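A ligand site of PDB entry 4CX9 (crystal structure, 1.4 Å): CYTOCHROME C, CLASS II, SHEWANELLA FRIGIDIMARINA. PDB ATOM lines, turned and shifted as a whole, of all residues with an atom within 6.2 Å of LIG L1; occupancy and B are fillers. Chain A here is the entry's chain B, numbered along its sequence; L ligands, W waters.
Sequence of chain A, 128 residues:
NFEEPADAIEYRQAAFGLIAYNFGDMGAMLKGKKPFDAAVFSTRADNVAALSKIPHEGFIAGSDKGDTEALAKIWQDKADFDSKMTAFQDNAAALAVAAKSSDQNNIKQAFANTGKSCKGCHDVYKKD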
ATOM      1  N   ALA A   8      23.532  31.780 -10.614  1.00  0.00           N
ATOM      2  CA  ALA A   8      23.371  30.442 -11.242  1.00  0.00           C
ATOM      3  C   ALA A   8      22.083  29.801 -10.781  1.00  0.00           C
ATOM      4  O   ALA A   8      21.381  29.161 -11.542  1.00  0.00           O
ATOM      5  CB  ALA A   8      24.572  29.594 -10.912  1.00  0.00           C
ATOM      6  N   ILE A   9      21.760  29.965  -9.492  1.00  0.00           N
ATOM      7  CA  ILE A   9      20.515  29.407  -8.938  1.00  0.00           C
ATOM      8  C   ILE A   9      19.330  30.090  -9.596  1.00  0.00           C
ATOM      9  O   ILE A   9      18.358  29.420  -9.998  1.00  0.00           O
ATOM     10  CB  ILE A   9      20.410  29.573  -7.397  1.00  0.00           C
ATOM     11  CG1 ILE A   9      21.452  28.663  -6.729  1.00  0.00           C
ATOM     12  CG2 ILE A   9      19.022  29.233  -6.889  1.00  0.00           C
ATOM     13  CD1 ILE A   9      21.801  29.062  -5.299  1.00  0.00           C
ATOM     14  N   ARG A  12      18.836  28.840 -13.261  1.00  0.00           N
ATOM     15  CA  ARG A  12      18.239  27.540 -13.432  1.00  0.00           C
ATOM     16  C   ARG A  12      16.791  27.443 -12.921  1.00  0.00           C
ATOM     17  O   ARG A  12      15.970  26.763 -13.520  1.00  0.00           O
ATOM     18  CB  ARG A  12      19.146  26.457 -12.824  1.00  0.00           C
ATOM     19  CG  ARG A  12      19.169  26.428 -11.290  1.00  0.00           C
ATOM     20  CD  ARG A  12      20.490  25.882 -10.809  1.00  0.00           C
ATOM     21  NE  ARG A  12      20.503  25.614  -9.352  1.00  0.00           N
ATOM     22  CZ  ARG A  12      21.630  25.492  -8.659  1.00  0.00           C
ATOM     23  NH1 ARG A  12      22.812  25.638  -9.236  1.00  0.00           N
ATOM     24  NH2 ARG A  12      21.558  25.194  -7.361  1.00  0.00           N
ATOM     25  N   GLN A  13      16.466  28.148 -11.824  1.00  0.00           N
ATOM     26  CA  GLN A  13      15.113  28.233 -11.331  1.00  0.00           C
ATOM     27  C   GLN A  13      14.166  28.927 -12.328  1.00  0.00           C
ATOM     28  O   GLN A  13      13.061  28.441 -12.624  1.00  0.00           O
ATOM     29  CB  GLN A  13      15.075  28.973  -9.982  1.00  0.00           C
ATOM     30  CG  GLN A  13      15.611  28.103  -8.865  1.00  0.00           C
ATOM     31  CD  GLN A  13      15.586  28.783  -7.514  1.00  0.00           C
ATOM     32  OE1 GLN A  13      15.537  30.011  -7.452  1.00  0.00           O
ATOM     33  NE2 GLN A  13      15.762  28.001  -6.440  1.00  0.00           N
ATOM     34  N   ALA A  14      14.657  30.010 -12.928  1.00  0.00           N
ATOM     35  CA  ALA A  14      13.841  30.721 -13.916  1.00  0.00           C
ATOM     36  C   ALA A  14      13.540  29.816 -15.087  1.00  0.00           C
ATOM     37  O   ALA A  14      12.384  29.718 -15.562  1.00  0.00           O
ATOM     38  CB  ALA A  14      14.572  31.955 -14.407  1.00  0.00           C
ATOM     39  N   PHE A  16      13.512  26.454 -15.223  1.00  0.00           N
ATOM     40  CA  PHE A  16      12.574  25.396 -14.915  1.00  0.00           C
ATOM     41  C   PHE A  16      11.171  25.912 -14.671  1.00  0.00           C
ATOM     42  O   PHE A  16      10.226  25.217 -14.986  1.00  0.00           O
ATOM     43  CB  PHE A  16      13.085  24.568 -13.723  1.00  0.00           C
ATOM     44  CG  PHE A  16      14.055  23.533 -14.102  1.00  0.00           C
ATOM     45  CD1 PHE A  16      13.731  22.549 -15.035  1.00  0.00           C
ATOM     46  CD2 PHE A  16      15.333  23.462 -13.500  1.00  0.00           C
ATOM     47  CE1 PHE A  16      14.647  21.545 -15.380  1.00  0.00           C
ATOM     48  CE2 PHE A  16      16.219  22.474 -13.870  1.00  0.00           C
ATOM     49  CZ  PHE A  16      15.867  21.526 -14.803  1.00  0.00           C
ATOM     50  N   GLY A  17      10.988  27.107 -14.087  1.00  0.00           N
ATOM     51  CA  GLY A  17       9.664  27.675 -13.973  1.00  0.00           C
ATOM     52  C   GLY A  17       8.964  27.915 -15.312  1.00  0.00           C
ATOM     53  O   GLY A  17       7.791  27.589 -15.483  1.00  0.00           O
ATOM     54  N   ILE A  19       9.773  26.194 -18.073  1.00  0.00           N
ATOM     55  CA  ILE A  19       9.516  24.835 -18.537  1.00  0.00           C
ATOM     56  C   ILE A  19       8.209  24.319 -17.977  1.00  0.00           C
ATOM     57  O   ILE A  19       7.411  23.762 -18.705  1.00  0.00           O
ATOM     58  CB  ILE A  19      10.719  23.903 -18.187  1.00  0.00           C
ATOM     59  CG1 ILE A  19      11.902  24.270 -19.071  1.00  0.00           C
ATOM     60  CG2 ILE A  19      10.340  22.438 -18.324  1.00  0.00           C
ATOM     61  CD1 ILE A  19      13.238  23.685 -18.629  1.00  0.00           C
ATOM     62  N   ALA A  20       8.033  24.473 -16.670  1.00  0.00           N
ATOM     63  CA  ALA A  20       6.872  23.842 -15.963  1.00  0.00           C
ATOM     64  C   ALA A  20       5.556  24.484 -16.466  1.00  0.00           C
ATOM     65  O   ALA A  20       4.576  23.809 -16.646  1.00  0.00           O
ATOM     66  CB  ALA A  20       7.036  24.089 -14.482  1.00  0.00           C
ATOM     67  N   PHE A  23       5.095  23.111 -20.125  1.00  0.00           N
ATOM     68  CA  PHE A  23       4.816  21.687 -20.058  1.00  0.00           C
ATOM     69  C   PHE A  23       3.433  21.406 -19.430  1.00  0.00           C
ATOM     70  O   PHE A  23       2.694  20.516 -19.901  1.00  0.00           O
ATOM     71  CB  PHE A  23       5.923  21.013 -19.234  1.00  0.00           C
ATOM     72  CG  PHE A  23       5.923  19.497 -19.347  1.00  0.00           C
ATOM     73  CD1 PHE A  23       6.344  18.885 -20.484  1.00  0.00           C
ATOM     74  CD2 PHE A  23       5.449  18.740 -18.303  1.00  0.00           C
ATOM     75  CE1 PHE A  23       6.338  17.518 -20.597  1.00  0.00           C
ATOM     76  CE2 PHE A  23       5.419  17.344 -18.436  1.00  0.00           C
ATOM     77  CZ  PHE A  23       5.855  16.772 -19.580  1.00  0.00           C
ATOM     78  N   VAL A  48       9.172  24.110 -24.698  1.00  0.00           N
ATOM     79  CA  VAL A  48       9.827  23.183 -23.772  1.00  0.00           C
ATOM     80  C   VAL A  48      11.133  22.676 -24.380  1.00  0.00           C
ATOM     81  O   VAL A  48      12.144  22.560 -23.697  1.00  0.00           O
ATOM     82  CB  VAL A  48       8.862  22.044 -23.286  1.00  0.00           C
ATOM     83  CG1 VAL A  48       9.644  20.992 -22.518  1.00  0.00           C
ATOM     84  CG2 VAL A  48       7.754  22.634 -22.435  1.00  0.00           C
ATOM     85  N   PHE A  59      23.990  24.700 -13.047  1.00  0.00           N
ATOM     86  CA  PHE A  59      24.377  23.708 -11.997  1.00  0.00           C
ATOM     87  C   PHE A  59      25.888  23.683 -11.760  1.00  0.00           C
ATOM     88  O   PHE A  59      26.552  22.633 -11.930  1.00  0.00           O
ATOM     89  CB  PHE A  59      23.767  22.347 -12.267  1.00  0.00           C
ATOM     90  CG  PHE A  59      22.272  22.338 -12.092  1.00  0.00           C
ATOM     91  CD1 PHE A  59      21.713  22.170 -10.823  1.00  0.00           C
ATOM     92  CD2 PHE A  59      21.406  22.573 -13.146  1.00  0.00           C
ATOM     93  CE1 PHE A  59      20.336  22.179 -10.636  1.00  0.00           C
ATOM     94  CE2 PHE A  59      20.031  22.579 -12.972  1.00  0.00           C
ATOM     95  CZ  PHE A  59      19.483  22.413 -11.694  1.00  0.00           C
ATOM     96  N   SER A  63      27.130  25.523  -5.700  1.00  0.00           N
ATOM     97  CA  SER A  63      25.844  26.231  -5.723  1.00  0.00           C
ATOM     98  C   SER A  63      24.709  25.417  -5.062  1.00  0.00           C
ATOM     99  O   SER A  63      23.551  25.578  -5.430  1.00  0.00           O
ATOM    100  CB  SER A  63      25.477  26.625  -7.143  1.00  0.00           C
ATOM    101  OG  SER A  63      25.263  25.498  -7.944  1.00  0.00           O
ATOM    102  N   ASP A  67      19.301  29.606  -1.154  1.00  0.00           N
ATOM    103  CA  ASP A  67      17.920  29.456  -1.507  1.00  0.00           C
ATOM    104  C   ASP A  67      17.826  28.647  -2.814  1.00  0.00           C
ATOM    105  O   ASP A  67      17.528  29.180  -3.875  1.00  0.00           O
ATOM    106  CB  ASP A  67      17.236  30.803  -1.628  1.00  0.00           C
ATOM    107  CG  ASP A  67      15.802  30.686  -2.083  1.00  0.00           C
ATOM    108  OD1 ASP A  67      15.170  29.685  -1.740  1.00  0.00           O
ATOM    109  OD2 ASP A  67      15.252  31.612  -2.757  1.00  0.00           O
ATOM    110  N   THR A  68      18.012  27.348  -2.696  1.00  0.00           N
ATOM    111  CA  THR A  68      17.939  26.416  -3.828  1.00  0.00           C
ATOM    112  C   THR A  68      17.324  25.137  -3.362  1.00  0.00           C
ATOM    113  O   THR A  68      17.509  24.741  -2.195  1.00  0.00           O
ATOM    114  CB  THR A  68      19.345  26.181  -4.452  1.00  0.00           C
ATOM    115  OG1 THR A  68      19.231  25.262  -5.551  1.00  0.00           O
ATOM    116  CG2 THR A  68      20.330  25.642  -3.433  1.00  0.00           C
ATOM    117  N   GLU A  69      16.616  24.454  -4.248  1.00  0.00           N
ATOM    118  CA  GLU A  69      16.094  23.126  -3.988  1.00  0.00           C
ATOM    119  C   GLU A  69      17.007  22.021  -4.568  1.00  0.00           C
ATOM    120  O   GLU A  69      16.666  20.855  -4.533  1.00  0.00           O
ATOM    121  CB  GLU A  69      14.706  22.996  -4.593  1.00  0.00           C
ATOM    122  CG  GLU A  69      13.779  24.127  -4.170  1.00  0.00           C
ATOM    123  CD  GLU A  69      13.604  24.223  -2.692  1.00  0.00           C
ATOM    124  OE1 GLU A  69      13.126  23.237  -2.135  1.00  0.00           O
ATOM    125  OE2 GLU A  69      13.987  25.252  -2.084  1.00  0.00           O
ATOM    126  N   ALA A  70      18.119  22.441  -5.161  1.00  0.00           N
ATOM    127  CA  ALA A  70      19.101  21.474  -5.694  1.00  0.00           C
ATOM    128  C   ALA A  70      19.780  20.761  -4.533  1.00  0.00           C
ATOM    129  O   ALA A  70      20.264  21.416  -3.620  1.00  0.00           O
ATOM    130  CB  ALA A  70      20.150  22.207  -6.531  1.00  0.00           C
ATOM    131  N   LEU A  71      19.853  19.433  -4.595  1.00  0.00           N
ATOM    132  CA  LEU A  71      20.603  18.664  -3.591  1.00  0.00           C
ATOM    133  C   LEU A  71      22.103  18.583  -3.869  1.00  0.00           C
ATOM    134  O   LEU A  71      22.543  18.542  -5.030  1.00  0.00           O
ATOM    135  CB  LEU A  71      20.006  17.268  -3.478  1.00  0.00           C
ATOM    136  CG  LEU A  71      18.540  17.159  -3.110  1.00  0.00           C
ATOM    137  CD1 LEU A  71      18.031  15.738  -3.151  1.00  0.00           C
ATOM    138  CD2 LEU A  71      18.325  17.804  -1.738  1.00  0.00           C
ATOM    139  N   ILE A  74      23.641  16.091  -6.566  1.00  0.00           N
ATOM    140  CA  ILE A  74      23.915  16.458  -7.965  1.00  0.00           C
ATOM    141  C   ILE A  74      25.414  16.404  -8.227  1.00  0.00           C
ATOM    142  O   ILE A  74      25.843  15.899  -9.270  1.00  0.00           O
ATOM    143  CB  ILE A  74      23.329  17.845  -8.291  1.00  0.00           C
ATOM    144  CG1 ILE A  74      21.788  17.774  -8.266  1.00  0.00           C
ATOM    145  CG2 ILE A  74      23.853  18.350  -9.634  1.00  0.00           C
ATOM    146  CD1 ILE A  74      21.156  19.161  -8.394  1.00  0.00           C
ATOM    147  N   PHE A  81      23.357  12.823 -13.104  1.00  0.00           N
ATOM    148  CA  PHE A  81      22.526  14.027 -13.302  1.00  0.00           C
ATOM    149  C   PHE A  81      22.564  14.438 -14.790  1.00  0.00           C
ATOM    150  O   PHE A  81      21.540  14.724 -15.384  1.00  0.00           O
ATOM    151  CB  PHE A  81      23.018  15.149 -12.427  1.00  0.00           C
ATOM    152  CG  PHE A  81      22.228  16.430 -12.539  1.00  0.00           C
ATOM    153  CD1 PHE A  81      21.077  16.630 -11.795  1.00  0.00           C
ATOM    154  CD2 PHE A  81      22.721  17.476 -13.308  1.00  0.00           C
ATOM    155  CE1 PHE A  81      20.385  17.850 -11.872  1.00  0.00           C
ATOM    156  CE2 PHE A  81      22.030  18.679 -13.381  1.00  0.00           C
ATOM    157  CZ  PHE A  81      20.884  18.883 -12.644  1.00  0.00           C
ATOM    158  N   ASP A  82      23.775  14.481 -15.352  1.00  0.00           N
ATOM    159  CA  ASP A  82      23.983  14.921 -16.715  1.00  0.00           C
ATOM    160  C   ASP A  82      23.305  13.974 -17.731  1.00  0.00           C
ATOM    161  O   ASP A  82      22.679  14.436 -18.686  1.00  0.00           O
ATOM    162  CB  ASP A  82      25.481  15.014 -17.029  1.00  0.00           C
ATOM    163  CG  ASP A  82      26.170  16.170 -16.373  1.00  0.00           C
ATOM    164  OD1 ASP A  82      25.511  17.058 -15.776  1.00  0.00           O
ATOM    165  OD2 ASP A  82      27.430  16.284 -16.534  1.00  0.00           O
ATOM    166  N   LYS A  84      20.602  12.135 -17.071  1.00  0.00           N
ATOM    167  CA  LYS A  84      19.174  12.480 -16.983  1.00  0.00           C
ATOM    168  C   LYS A  84      18.843  13.766 -17.714  1.00  0.00           C
ATOM    169  O   LYS A  84      17.806  13.844 -18.357  1.00  0.00           O
ATOM    170  CB  LYS A  84      18.726  12.590 -15.544  1.00  0.00           C
ATOM    171  CG  LYS A  84      18.703  11.247 -14.813  1.00  0.00           C
ATOM    172  CD  LYS A  84      18.157  11.417 -13.408  1.00  0.00           C
ATOM    173  CE  LYS A  84      18.197  10.190 -12.484  1.00  0.00           C
ATOM    174  NZ  LYS A  84      17.612   9.059 -13.147  1.00  0.00           N
ATOM    175  N   MET A  85      19.697  14.798 -17.596  1.00  0.00           N
ATOM    176  CA  MET A  85      19.423  16.054 -18.263  1.00  0.00           C
ATOM    177  C   MET A  85      19.458  15.894 -19.769  1.00  0.00           C
ATOM    178  O   MET A  85      18.563  16.397 -20.485  1.00  0.00           O
ATOM    179  CB  MET A  85      20.448  17.089 -17.858  1.00  0.00           C
ATOM    180  CG  MET A  85      20.164  18.483 -18.398  1.00  0.00           C
ATOM    181  SD  MET A  85      18.737  19.268 -17.622  1.00  0.00           S
ATOM    182  CE  MET A  85      19.452  19.815 -16.063  1.00  0.00           C
ATOM    183  N   THR A  86      20.453  15.170 -20.262  1.00  0.00           N
ATOM    184  CA  THR A  86      20.503  14.897 -21.700  1.00  0.00           C
ATOM    185  C   THR A  86      19.280  14.134 -22.212  1.00  0.00           C
ATOM    186  O   THR A  86      18.687  14.459 -23.291  1.00  0.00           O
ATOM    187  CB  THR A  86      21.803  14.165 -22.061  1.00  0.00           C
ATOM    188  OG1 THR A  86      22.929  14.991 -21.717  1.00  0.00           O
ATOM    189  CG2 THR A  86      21.805  13.826 -23.545  1.00  0.00           C
ATOM    190  N   PHE A  88      16.379  14.112 -20.878  1.00  0.00           N
ATOM    191  CA  PHE A  88      15.267  15.088 -20.894  1.00  0.00           C
ATOM    192  C   PHE A  88      15.277  15.951 -22.141  1.00  0.00           C
ATOM    193  O   PHE A  88      14.242  16.138 -22.773  1.00  0.00           O
ATOM    194  CB  PHE A  88      15.345  15.914 -19.616  1.00  0.00           C
ATOM    195  CG  PHE A  88      14.516  17.179 -19.644  1.00  0.00           C
ATOM    196  CD1 PHE A  88      13.159  17.132 -19.921  1.00  0.00           C
ATOM    197  CD2 PHE A  88      15.082  18.396 -19.326  1.00  0.00           C
ATOM    198  CE1 PHE A  88      12.394  18.271 -19.934  1.00  0.00           C
ATOM    199  CE2 PHE A  88      14.324  19.541 -19.316  1.00  0.00           C
ATOM    200  CZ  PHE A  88      12.979  19.480 -19.647  1.00  0.00           C
ATOM    201  N   THR A 114       8.664  12.403 -21.689  1.00  0.00           N
ATOM    202  CA  THR A 114       9.248  13.648 -21.166  1.00  0.00           C
ATOM    203  C   THR A 114       8.904  13.845 -19.697  1.00  0.00           C
ATOM    204  O   THR A 114       9.741  14.214 -18.886  1.00  0.00           O
ATOM    205  CB  THR A 114       8.804  14.864 -21.978  1.00  0.00           C
ATOM    206  OG1 THR A 114       9.149  14.678 -23.331  1.00  0.00           O
ATOM    207  CG2 THR A 114       9.526  16.114 -21.421  1.00  0.00           C
ATOM    208  N   GLY A 115       7.662  13.564 -19.322  1.00  0.00           N
ATOM    209  CA  GLY A 115       7.241  13.656 -17.954  1.00  0.00           C
ATOM    210  C   GLY A 115       7.987  12.749 -17.006  1.00  0.00           C
ATOM    211  O   GLY A 115       8.303  13.171 -15.886  1.00  0.00           O
ATOM    212  N   SER A 117      11.046  11.912 -17.379  1.00  0.00           N
ATOM    213  CA  SER A 117      12.297  12.650 -17.091  1.00  0.00           C
ATOM    214  C   SER A 117      12.199  13.584 -15.958  1.00  0.00           C
ATOM    215  O   SER A 117      13.100  13.698 -15.153  1.00  0.00           O
ATOM    216  CB  SER A 117      12.784  13.420 -18.321  1.00  0.00           C
ATOM    217  OG  SER A 117      13.223  12.535 -19.292  1.00  0.00           O
ATOM    218  N   CYS A 118      11.139  14.395 -15.923  1.00  0.00           N
ATOM    219  CA  CYS A 118      11.004  15.317 -14.810  1.00  0.00           C
ATOM    220  C   CYS A 118      11.007  14.600 -13.483  1.00  0.00           C
ATOM    221  O   CYS A 118      11.666  14.999 -12.538  1.00  0.00           O
ATOM    222  CB  CYS A 118       9.678  16.097 -14.874  1.00  0.00           C
ATOM    223  SG  CYS A 118       9.097  16.679 -16.502  1.00  0.00           S
ATOM    224  N   LYS A 119      10.198  13.561 -13.398  1.00  0.00           N
ATOM    225  CA  LYS A 119       9.993  12.898 -12.120  1.00  0.00           C
ATOM    226  C   LYS A 119      11.261  12.173 -11.659  1.00  0.00           C
ATOM    227  O   LYS A 119      11.588  12.212 -10.479  1.00  0.00           O
ATOM    228  CB  LYS A 119       8.858  11.890 -12.236  1.00  0.00           C
ATOM    229  CG  LYS A 119       8.626  11.036 -11.007  1.00  0.00           C
ATOM    230  CD  LYS A 119       7.477  10.065 -11.261  1.00  0.00           C
ATOM    231  CE  LYS A 119       7.425   8.958 -10.252  1.00  0.00           C
ATOM    232  NZ  LYS A 119       7.033   9.551  -8.956  1.00  0.00           N
ATOM    233  N   CYS A 121      14.386  12.786 -12.289  1.00  0.00           N
ATOM    234  CA  CYS A 121      15.350  13.680 -11.750  1.00  0.00           C
ATOM    235  C   CYS A 121      14.916  14.326 -10.453  1.00  0.00           C
ATOM    236  O   CYS A 121      15.697  14.400  -9.485  1.00  0.00           O
ATOM    237  CB  CYS A 121      15.745  14.700 -12.808  1.00  0.00           C
ATOM    238  SG  CYS A 121      17.140  15.655 -12.306  1.00  0.00           S
ATOM    239  N   HIS A 122      13.666  14.812 -10.415  1.00  0.00           N
ATOM    240  CA  HIS A 122      13.070  15.326  -9.201  1.00  0.00           C
ATOM    241  C   HIS A 122      13.295  14.392  -7.977  1.00  0.00           C
ATOM    242  O   HIS A 122      13.767  14.865  -6.933  1.00  0.00           O
ATOM    243  CB  HIS A 122      11.555  15.540  -9.441  1.00  0.00           C
ATOM    244  CG  HIS A 122      10.791  15.945  -8.221  1.00  0.00           C
ATOM    245  ND1 HIS A 122      10.097  15.031  -7.452  1.00  0.00           N
ATOM    246  CD2 HIS A 122      10.578  17.156  -7.662  1.00  0.00           C
ATOM    247  CE1 HIS A 122       9.523  15.662  -6.440  1.00  0.00           C
ATOM    248  NE2 HIS A 122       9.805  16.952  -6.540  1.00  0.00           N
ATOM    249  N   TYR A 125      17.328  14.324  -7.169  1.00  0.00           N
ATOM    250  CA  TYR A 125      18.204  15.487  -7.122  1.00  0.00           C
ATOM    251  C   TYR A 125      17.572  16.790  -6.606  1.00  0.00           C
ATOM    252  O   TYR A 125      18.289  17.776  -6.490  1.00  0.00           O
ATOM    253  CB  TYR A 125      18.820  15.713  -8.520  1.00  0.00           C
ATOM    254  CG  TYR A 125      19.731  14.586  -8.925  1.00  0.00           C
ATOM    255  CD1 TYR A 125      20.929  14.378  -8.270  1.00  0.00           C
ATOM    256  CD2 TYR A 125      19.383  13.716  -9.973  1.00  0.00           C
ATOM    257  CE1 TYR A 125      21.787  13.324  -8.644  1.00  0.00           C
ATOM    258  CE2 TYR A 125      20.262  12.695 -10.381  1.00  0.00           C
ATOM    259  CZ  TYR A 125      21.423  12.458  -9.674  1.00  0.00           C
ATOM    260  OH  TYR A 125      22.297  11.409  -9.979  1.00  0.00           O
ATOM    261  N   LYS A 126      16.278  16.777  -6.277  1.00  0.00           N
ATOM    262  CA  LYS A 126      15.606  17.976  -5.795  1.00  0.00           C
ATOM    263  C   LYS A 126      15.041  17.705  -4.413  1.00  0.00           C
ATOM    264  O   LYS A 126      14.597  16.608  -4.142  1.00  0.00           O
ATOM    265  CB  LYS A 126      14.491  18.401  -6.754  1.00  0.00           C
ATOM    266  CG  LYS A 126      13.869  19.774  -6.490  1.00  0.00           C
ATOM    267  CD  LYS A 126      12.876  20.103  -7.608  1.00  0.00           C
ATOM    268  CE  LYS A 126      12.122  21.391  -7.432  1.00  0.00           C
ATOM    269  NZ  LYS A 126      11.110  21.308  -6.329  1.00  0.00           N
HETATM  270 FE1  LIG L   1      12.954  20.236 -12.539  1.00  0.00          FE
HETATM  271  C1  LIG L   1      13.427  22.725 -10.278  1.00  0.00           C
HETATM  272  C2  LIG L   1       9.861  21.385 -13.178  1.00  0.00           C
HETATM  273  C3  LIG L   1      12.827  18.391 -15.374  1.00  0.00           C
HETATM  274  C4  LIG L   1      15.993  19.079 -11.901  1.00  0.00           C
HETATM  275  N1  LIG L   1      11.872  21.786 -11.849  1.00  0.00           N
HETATM  276  C5  LIG L   1      12.192  22.694 -10.935  1.00  0.00           C
HETATM  277  C6  LIG L   1      11.098  23.560 -10.675  1.00  0.00           C
HETATM  278  C7  LIG L   1      10.087  23.132 -11.441  1.00  0.00           C
HETATM  279  C8  LIG L   1      10.574  22.076 -12.189  1.00  0.00           C
HETATM  280  C9  LIG L   1       8.712  23.726 -11.551  1.00  0.00           C
HETATM  281  C10 LIG L   1      11.087  24.690  -9.720  1.00  0.00           C
HETATM  282  C11 LIG L   1      11.633  25.969 -10.372  1.00  0.00           C
HETATM  283  C12 LIG L   1      11.615  27.144  -9.422  1.00  0.00           C
HETATM  284  O1  LIG L   1      12.465  27.285  -8.531  1.00  0.00           O
HETATM  285  O2  LIG L   1      10.710  27.989  -9.556  1.00  0.00           O
HETATM  286  N2  LIG L   1      11.605  19.912 -14.001  1.00  0.00           N
HETATM  287  C13 LIG L   1      10.320  20.412 -14.048  1.00  0.00           C
HETATM  288  C14 LIG L   1       9.586  19.858 -15.082  1.00  0.00           C
HETATM  289  C15 LIG L   1      10.428  19.028 -15.745  1.00  0.00           C
HETATM  290  C16 LIG L   1      11.649  19.082 -15.045  1.00  0.00           C
HETATM  291  C17 LIG L   1       8.139  20.111 -15.414  1.00  0.00           C
HETATM  292  C18 LIG L   1      10.209  18.183 -16.972  1.00  0.00           C
HETATM  293  C19 LIG L   1       9.441  18.809 -18.138  1.00  0.00           C
HETATM  294  N3  LIG L   1      14.203  18.957 -13.467  1.00  0.00           N
HETATM  295  C20 LIG L   1      13.996  18.273 -14.621  1.00  0.00           C
HETATM  296  C21 LIG L   1      15.087  17.428 -14.938  1.00  0.00           C
HETATM  297  C22 LIG L   1      16.018  17.602 -13.942  1.00  0.00           C
HETATM  298  C23 LIG L   1      15.421  18.541 -13.054  1.00  0.00           C
HETATM  299  C24 LIG L   1      15.126  16.517 -16.141  1.00  0.00           C
HETATM  300  C25 LIG L   1      17.401  16.995 -13.737  1.00  0.00           C
HETATM  301  C26 LIG L   1      18.071  16.294 -14.897  1.00  0.00           C
HETATM  302  N4  LIG L   1      14.377  20.838 -11.351  1.00  0.00           N
HETATM  303  C27 LIG L   1      15.552  20.159 -11.105  1.00  0.00           C
HETATM  304  C28 LIG L   1      16.302  20.639 -10.035  1.00  0.00           C
HETATM  305  C29 LIG L   1      15.620  21.739  -9.591  1.00  0.00           C
HETATM  306  C30 LIG L   1      14.450  21.767 -10.397  1.00  0.00           C
HETATM  307  C31 LIG L   1      17.582  20.059  -9.495  1.00  0.00           C
HETATM  308  C32 LIG L   1      15.969  22.757  -8.497  1.00  0.00           C
HETATM  309  C33 LIG L   1      16.640  24.025  -9.038  1.00  0.00           C
HETATM  310  C34 LIG L   1      17.040  24.956  -7.891  1.00  0.00           C
HETATM  311  O3  LIG L   1      16.149  25.096  -6.981  1.00  0.00           O
HETATM  312  O4  LIG L   1      18.154  25.528  -7.851  1.00  0.00           O
HETATM  313  N1  LG2 L   2      12.158  18.946 -11.379  1.00  0.00           N
HETATM  314  O1  LG2 L   2      12.927  18.250 -10.783  1.00  0.00           O
HETATM  315  O   HOH W   1      13.422  25.019  -7.468  1.00  0.00           O
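The guanidinium group (NE) of Arg 12 lies within salt-bridge range of an oxygen (O4) of LIG L1.
The side-chain sulfur (SG) of Cys 121 is bonded to a carbon (C25) of LIG L1 (2.0 Å).
O4 of LIG L1 sits at hydrogen-bond distance from OG1 of Thr 68, 2.6 Å away.
C18 of LIG L1 is covalently linked to SG of Cys 118 (1.9 Å).
The backbone NH of Glu 69 lies within hydrogen-bond range of an oxygen (O3) of LIG L1, 2.8 Å away.
The side-chain amide nitrogen (NE2) of Gln 13 is in hydrogen-bond range of an oxygen (O3) of LIG L1 (3.0 Å).
An iron atom (FE1) of LIG L1 is bound by a nitrogen (N1) of LG2 L2.
NE2 of Gln 13 sits at hydrogen-bond distance from O of Asp 67, 3.3 Å away.
The side-chain hydroxyl (OG1) of Thr 68 sits at hydrogen-bond distance from the guanidinium group (NH2) of Arg 12.
N of Leu 71 lies within hydrogen-bond range of O of Tyr 125 (3.0 Å).
The side-chain hydroxyl (OG1) of Thr 68 is in hydrogen-bond range of the backbone NH (N) of Ala 70 (3.1 Å).
NH1 of Arg 12 is in hydrogen-bond range of OG of Ser 63 (2.8 Å).
CG2 of Ile 9 touches O4 of LIG L1, 3.9 Å away.
Phe 16 touches LIG L1 (CE1 to N3, 3.2 Å).
Gly 17 touches LIG L1 (N to C11, 3.9 Å).
Ile 19 touches LIG L1 (CG2 to C19, 3.7 Å).
CB of Ala 20 touches C9 of LIG L1, at 3.4 Å.
Phe 23 touches LIG L1 (CG to C19, 3.8 Å).
CE1 of Phe 59 touches C31 of LIG L1, 3.7 Å away.
Ala 70 touches LIG L1 (N to O3, 3.8 Å).
Ile 74 touches LIG L1 (CD1 to C31, 3.8 Å).
Phe 81 touches LIG L1.
CB of Lys 84 touches C26 of LIG L1, at 3.8 Å.
N of Met 85 touches C26 of LIG L1, 3.5 Å away.
Phe 88 touches LIG L1.
Ser 117 touches LIG L1 (O to C24, 3.6 Å).
Tyr 125 touches LIG L1 (O to C31, 3.8 Å).
Lys 126 touches LIG L1.
Hydrophobic or aromatic side chains within 4 Å of LIG L1: Ile 9, Phe 16, Ile 19, Ala 20, Phe 23, Phe 59, Ile 74, Phe 81, Met 85 and Phe 88.
Of the 34 residues printed, 22 come within 4 Å of LIG L1.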
